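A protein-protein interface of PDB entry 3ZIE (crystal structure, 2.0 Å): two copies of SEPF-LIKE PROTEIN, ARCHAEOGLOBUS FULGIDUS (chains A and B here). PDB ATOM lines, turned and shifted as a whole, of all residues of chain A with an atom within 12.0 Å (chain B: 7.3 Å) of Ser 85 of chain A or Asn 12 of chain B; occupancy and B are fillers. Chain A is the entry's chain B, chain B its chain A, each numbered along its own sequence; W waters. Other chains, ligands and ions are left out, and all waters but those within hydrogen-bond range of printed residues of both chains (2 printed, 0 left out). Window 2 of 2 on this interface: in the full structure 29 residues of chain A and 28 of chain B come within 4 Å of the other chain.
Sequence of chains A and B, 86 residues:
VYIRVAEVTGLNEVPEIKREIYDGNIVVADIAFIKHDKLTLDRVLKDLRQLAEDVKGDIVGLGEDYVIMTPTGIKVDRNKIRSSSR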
ATOM      1  N   LYS A  80      -4.757   4.671  19.820  1.00  0.00           N
ATOM      2  CA  LYS A  80      -4.913   6.016  20.401  1.00  0.00           C
ATOM      3  C   LYS A  80      -3.993   6.249  21.584  1.00  0.00           C
ATOM      4  O   LYS A  80      -3.505   5.292  22.194  1.00  0.00           O
ATOM      5  CB  LYS A  80      -6.374   6.245  20.784  1.00  0.00           C
ATOM      6  CG  LYS A  80      -7.205   6.334  19.501  1.00  0.00           C
ATOM      7  CD  LYS A  80      -8.662   6.369  19.732  1.00  0.00           C
ATOM      8  CE  LYS A  80      -9.313   5.997  18.390  1.00  0.00           C
ATOM      9  NZ  LYS A  80     -10.580   6.633  18.473  1.00  0.00           N
ATOM     10  N   ILE A  81      -3.780   7.510  21.918  1.00  0.00           N
ATOM     11  CA  ILE A  81      -3.186   7.872  23.214  1.00  0.00           C
ATOM     12  C   ILE A  81      -4.304   7.863  24.224  1.00  0.00           C
ATOM     13  O   ILE A  81      -5.348   8.498  24.008  1.00  0.00           O
ATOM     14  CB  ILE A  81      -2.565   9.298  23.175  1.00  0.00           C
ATOM     15  CG1 ILE A  81      -1.417   9.352  22.145  1.00  0.00           C
ATOM     16  CG2 ILE A  81      -2.098   9.720  24.615  1.00  0.00           C
ATOM     17  CD1 ILE A  81      -0.924  10.861  21.811  1.00  0.00           C
ATOM     18  N   ARG A  82      -4.096   7.141  25.313  1.00  0.00           N
ATOM     19  CA  ARG A  82      -5.085   7.059  26.359  1.00  0.00           C
ATOM     20  C   ARG A  82      -4.403   7.323  27.690  1.00  0.00           C
ATOM     21  O   ARG A  82      -3.165   7.398  27.790  1.00  0.00           O
ATOM     22  CB  ARG A  82      -5.763   5.680  26.367  1.00  0.00           C
ATOM     23  CG  ARG A  82      -6.623   5.403  25.121  1.00  0.00           C
ATOM     24  CD  ARG A  82      -7.178   3.960  25.097  1.00  0.00           C
ATOM     25  NE  ARG A  82      -7.962   3.657  23.879  1.00  0.00           N
ATOM     26  CZ  ARG A  82      -9.200   4.093  23.641  1.00  0.00           C
ATOM     27  NH1 ARG A  82      -9.846   4.873  24.515  1.00  0.00           N
ATOM     28  NH2 ARG A  82      -9.808   3.759  22.512  1.00  0.00           N
ATOM     29  N   SER A  83      -5.223   7.471  28.724  1.00  0.00           N
ATOM     30  CA  SER A  83      -4.748   7.728  30.076  1.00  0.00           C
ATOM     31  C   SER A  83      -3.561   6.798  30.413  1.00  0.00           C
ATOM     32  O   SER A  83      -3.612   5.589  30.123  1.00  0.00           O
ATOM     33  CB  SER A  83      -5.922   7.532  31.060  1.00  0.00           C
ATOM     34  OG  SER A  83      -5.439   7.572  32.385  1.00  0.00           O
ATOM     35  N   SER A  84      -2.490   7.370  30.970  1.00  0.00           N
ATOM     36  CA  SER A  84      -1.354   6.576  31.446  1.00  0.00           C
ATOM     37  C   SER A  84      -1.680   5.802  32.751  1.00  0.00           C
ATOM     38  O   SER A  84      -1.054   4.773  33.047  1.00  0.00           O
ATOM     39  CB  SER A  84      -0.123   7.462  31.631  1.00  0.00           C
ATOM     40  OG  SER A  84      -0.394   8.522  32.523  1.00  0.00           O
ATOM     41  N   SER A  85      -2.685   6.283  33.494  1.00  0.00           N
ATOM     42  CA  SER A  85      -3.140   5.647  34.750  1.00  0.00           C
ATOM     43  C   SER A  85      -3.961   4.401  34.460  1.00  0.00           C
ATOM     44  O   SER A  85      -3.515   3.292  34.737  1.00  0.00           O
ATOM     45  CB  SER A  85      -3.962   6.629  35.592  1.00  0.00           C
ATOM     46  OG  SER A  85      -3.435   7.955  35.494  1.00  0.00           O
ATOM     47  N   GLU B   7      -7.267  10.526  23.279  1.00  0.00           N
ATOM     48  CA  GLU B   7      -8.553  10.692  23.964  1.00  0.00           C
ATOM     49  C   GLU B   7      -8.261  11.380  25.251  1.00  0.00           C
ATOM     50  O   GLU B   7      -7.713  10.787  26.177  1.00  0.00           O
ATOM     51  CB  GLU B   7      -9.246   9.341  24.200  1.00  0.00           C
ATOM     52  CG  GLU B   7      -9.472   8.542  22.898  1.00  0.00           C
ATOM     53  CD  GLU B   7     -10.428   9.222  21.909  1.00  0.00           C
ATOM     54  OE1 GLU B   7     -11.280  10.039  22.362  1.00  0.00           O
ATOM     55  OE2 GLU B   7     -10.325   8.970  20.673  1.00  0.00           O
ATOM     56  N   VAL B   8      -8.572  12.671  25.294  1.00  0.00           N
ATOM     57  CA  VAL B   8      -8.098  13.500  26.373  1.00  0.00           C
ATOM     58  C   VAL B   8      -9.168  13.549  27.457  1.00  0.00           C
ATOM     59  O   VAL B   8     -10.115  14.350  27.387  1.00  0.00           O
ATOM     60  CB  VAL B   8      -7.669  14.922  25.864  1.00  0.00           C
ATOM     61  CG1 VAL B   8      -7.254  15.799  27.030  1.00  0.00           C
ATOM     62  CG2 VAL B   8      -6.480  14.787  24.850  1.00  0.00           C
ATOM     63  N   THR B   9      -8.991  12.700  28.469  1.00  0.00           N
ATOM     64  CA  THR B   9      -9.953  12.577  29.596  1.00  0.00           C
ATOM     65  C   THR B   9      -9.531  13.362  30.834  1.00  0.00           C
ATOM     66  O   THR B   9     -10.262  13.431  31.783  1.00  0.00           O
ATOM     67  CB  THR B   9     -10.193  11.072  29.978  1.00  0.00           C
ATOM     68  OG1 THR B   9      -8.951  10.336  29.936  1.00  0.00           O
ATOM     69  CG2 THR B   9     -11.084  10.448  28.985  1.00  0.00           C
ATOM     70  N   GLY B  10      -8.373  13.997  30.824  1.00  0.00           N
ATOM     71  CA  GLY B  10      -7.845  14.542  32.065  1.00  0.00           C
ATOM     72  C   GLY B  10      -6.465  15.089  31.849  1.00  0.00           C
ATOM     73  O   GLY B  10      -6.144  15.432  30.735  1.00  0.00           O
ATOM     74  N   LEU B  11      -5.648  15.144  32.895  1.00  0.00           N
ATOM     75  CA  LEU B  11      -4.252  15.617  32.723  1.00  0.00           C
ATOM     76  C   LEU B  11      -3.271  14.540  32.326  1.00  0.00           C
ATOM     77  O   LEU B  11      -2.174  14.832  31.868  1.00  0.00           O
ATOM     78  CB  LEU B  11      -3.775  16.314  33.996  1.00  0.00           C
ATOM     79  CG  LEU B  11      -4.503  17.654  34.206  1.00  0.00           C
ATOM     80  CD1 LEU B  11      -4.446  17.935  35.727  1.00  0.00           C
ATOM     81  CD2 LEU B  11      -3.900  18.790  33.354  1.00  0.00           C
ATOM     82  N   ASN B  12      -3.706  13.294  32.377  1.00  0.00           N
ATOM     83  CA  ASN B  12      -2.788  12.175  32.200  1.00  0.00           C
ATOM     84  C   ASN B  12      -2.429  11.810  30.744  1.00  0.00           C
ATOM     85  O   ASN B  12      -1.776  10.819  30.525  1.00  0.00           O
ATOM     86  CB  ASN B  12      -3.283  10.959  33.002  1.00  0.00           C
ATOM     87  CG  ASN B  12      -3.200  11.184  34.522  1.00  0.00           C
ATOM     88  OD1 ASN B  12      -4.021  10.671  35.291  1.00  0.00           O
ATOM     89  ND2 ASN B  12      -2.184  11.908  34.955  1.00  0.00           N
ATOM     90  N   GLU B  13      -2.864  12.566  29.751  1.00  0.00           N
ATOM     91  CA  GLU B  13      -2.499  12.212  28.408  1.00  0.00           C
ATOM     92  C   GLU B  13      -1.494  13.250  27.866  1.00  0.00           C
ATOM     93  O   GLU B  13      -0.795  12.992  26.878  1.00  0.00           O
ATOM     94  CB  GLU B  13      -3.731  12.144  27.501  1.00  0.00           C
ATOM     95  CG  GLU B  13      -4.714  11.007  27.887  1.00  0.00           C
ATOM     96  CD  GLU B  13      -5.599  11.433  29.081  1.00  0.00           C
ATOM     97  OE1 GLU B  13      -6.114  12.575  29.130  1.00  0.00           O
ATOM     98  OE2 GLU B  13      -5.740  10.636  30.011  1.00  0.00           O
ATOM     99  N   VAL B  14      -1.417  14.389  28.549  1.00  0.00           N
ATOM    100  CA  VAL B  14      -0.491  15.462  28.111  1.00  0.00           C
ATOM    101  C   VAL B  14       0.998  15.009  27.929  1.00  0.00           C
ATOM    102  O   VAL B  14       1.579  15.332  26.911  1.00  0.00           O
ATOM    103  CB  VAL B  14      -0.587  16.713  29.002  1.00  0.00           C
ATOM    104  CG1 VAL B  14       0.618  17.666  28.714  1.00  0.00           C
ATOM    105  CG2 VAL B  14      -1.922  17.445  28.781  1.00  0.00           C
ATOM    106  N   PRO B  15       1.611  14.287  28.922  1.00  0.00           N
ATOM    107  CA  PRO B  15       3.022  13.827  28.702  1.00  0.00           C
ATOM    108  C   PRO B  15       3.259  13.065  27.388  1.00  0.00           C
ATOM    109  O   PRO B  15       4.258  13.301  26.727  1.00  0.00           O
ATOM    110  CB  PRO B  15       3.315  12.930  29.921  1.00  0.00           C
ATOM    111  CG  PRO B  15       2.376  13.593  31.054  1.00  0.00           C
ATOM    112  CD  PRO B  15       1.091  13.877  30.249  1.00  0.00           C
ATOM    113  N   GLU B  16       2.354  12.153  27.027  1.00  0.00           N
ATOM    114  CA  GLU B  16       2.502  11.391  25.789  1.00  0.00           C
ATOM    115  C   GLU B  16       2.252  12.245  24.532  1.00  0.00           C
ATOM    116  O   GLU B  16       2.917  12.045  23.506  1.00  0.00           O
ATOM    117  CB  GLU B  16       1.560  10.161  25.792  1.00  0.00           C
ATOM    118  CG  GLU B  16       1.621   9.352  24.525  1.00  0.00           C
ATOM    119  CD  GLU B  16       3.048   8.847  24.192  1.00  0.00           C
ATOM    120  OE1 GLU B  16       3.809   8.608  25.141  1.00  0.00           O
ATOM    121  OE2 GLU B  16       3.405   8.655  22.993  1.00  0.00           O
ATOM    122  N   ILE B  17       1.274  13.160  24.612  1.00  0.00           N
ATOM    123  CA  ILE B  17       1.027  14.107  23.503  1.00  0.00           C
ATOM    124  C   ILE B  17       2.308  14.881  23.240  1.00  0.00           C
ATOM    125  O   ILE B  17       2.748  14.964  22.077  1.00  0.00           O
ATOM    126  CB  ILE B  17      -0.175  15.034  23.765  1.00  0.00           C
ATOM    127  CG1 ILE B  17      -1.465  14.196  23.737  1.00  0.00           C
ATOM    128  CG2 ILE B  17      -0.202  16.302  22.764  1.00  0.00           C
ATOM    129  CD1 ILE B  17      -2.679  14.947  24.430  1.00  0.00           C
ATOM    130  N   VAL B  44      -5.260  21.564  30.652  1.00  0.00           N
ATOM    131  CA  VAL B  44      -4.737  20.855  29.501  1.00  0.00           C
ATOM    132  C   VAL B  44      -4.356  21.838  28.360  1.00  0.00           C
ATOM    133  O   VAL B  44      -3.326  21.664  27.723  1.00  0.00           O
ATOM    134  CB  VAL B  44      -5.770  19.877  28.959  1.00  0.00           C
ATOM    135  CG1 VAL B  44      -5.340  19.358  27.566  1.00  0.00           C
ATOM    136  CG2 VAL B  44      -5.925  18.686  29.946  1.00  0.00           C
HETATM  137  O   HOH W   1      -7.750   8.695  28.146  1.00  0.00           O
HETATM  138  O   HOH W   2      -0.813   8.726  27.902  1.00  0.00           O
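Of the 6 printed residues of chain A, 6 touch a printed residue of chain B.
Hydrophobic or aromatic side chains of chain A that line the printed part of chain B: Ile 81.
Printed residues of chain B that touch a printed residue of chain A: Glu 7, Asn 12, Glu 13, Glu 16 and Ile 17.
Among the printed residues, 8 pairs touch across the chains.
Among the printed residues, Asp or Glu carboxylates within 4 Å of a Lys or Arg side-chain nitrogen of the other chain: Lys 80 of chain A with Glu 7 of chain B.
Glu 16 of chain B touches Ile 81 of chain A (CG to CG2, 3.7 Å).
Ile 81 of chain A touches Ile 17 of chain B.
Glu 13 of chain B touches Arg 82 of chain A.
Water W2 lies within hydrogen-bond range of the backbone carbonyl oxygen (O) of Arg 82 of chain A (2.7 Å) and the backbone carbonyl oxygen (O) of Asn 12 of chain B (3.5 Å).
Water W1 lies within hydrogen-bond range of the side-chain hydroxyl of Thr 9 of chain B (2.7 Å), the backbone NH of Ser 83 of chain A (2.9 Å), the backbone carbonyl oxygen of Glu 7 of chain B (2.9 Å) and the side-chain carboxylate of Glu 13 of chain B (3.4 Å).
The backbone NH (N) of Thr 9 of chain B sits at hydrogen-bond distance from the side-chain carboxylate (OE1) of Glu 13 of chain B (3.0 Å).
The backbone NH (N) of Gly 10 of chain B is in hydrogen-bond range of the side-chain carboxylate (OE1) of Glu 13 of chain B (3.2 Å).
The side-chain hydroxyl (OG) of Ser 83 of chain A sits at hydrogen-bond distance from the backbone NH (N) of Ser 85 of chain A, 3.2 Å away.
No position is printed for both chains.
Of the 8 pairs that touch across the chains among the printed residues, none has its exchanged pair printed and touching as well.
The side-chain carboxylate (OE2) of Glu 13 of chain B lies close to the backbone NH (N) of Ser 83 of chain A.
The backbone carbonyl oxygen of Asn 12 of chain B sits at hydrogen-bond distance from the side-chain hydroxyl of Ser 84 of chain A (3.3 Å).
The side-chain amino group (NZ) of Lys 80 of chain A lies within salt-bridge range of the side-chain carboxylate (OE2) of Glu 7 of chain B (3.2 Å).
The backbone carbonyl oxygen of Ile 81 of chain A lies within hydrogen-bond range of the backbone NH of Glu 7 of chain B, at 2.9 Å.
The side-chain hydroxyl (OG) of Ser 85 of chain A is in hydrogen-bond range of the side-chain amide oxygen (OD1) of Asn 12 of chain B (2.8 Å).
Printed residues of chain B within 4 Å of Ser 83 of chain A: Glu 13 (3.1 Å).
Ser 85 of chain A touches just one residue of chain B: Asn 12.
Of chain A, only Ser 84 (3.3 Å) and Ser 85 (2.8 Å) come within 4 Å of Asn 12 of chain B.
Glu 13 of chain B touches just these residues of chain A: Arg 82 and Ser 83.
No residue of chain A comes within 4 Å of Val 14 of chain B.
No residue of chain A comes within 4 Å of Pro 15 of chain B.
Of the printed residues of chain A, Ile 17 of chain B touches Ile 81.
The nearest residue of chain B that does not touch Ser 85 of chain A is Glu 13 of chain B (6.4 Å).
The nearest residue of chain A that does not touch Asn 12 of chain B is Ser 83 of chain A (4.1 Å).
The nearest printed residue of chain B that does not touch Ser 83 of chain A is Asn 12 of chain B (4.1 Å).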
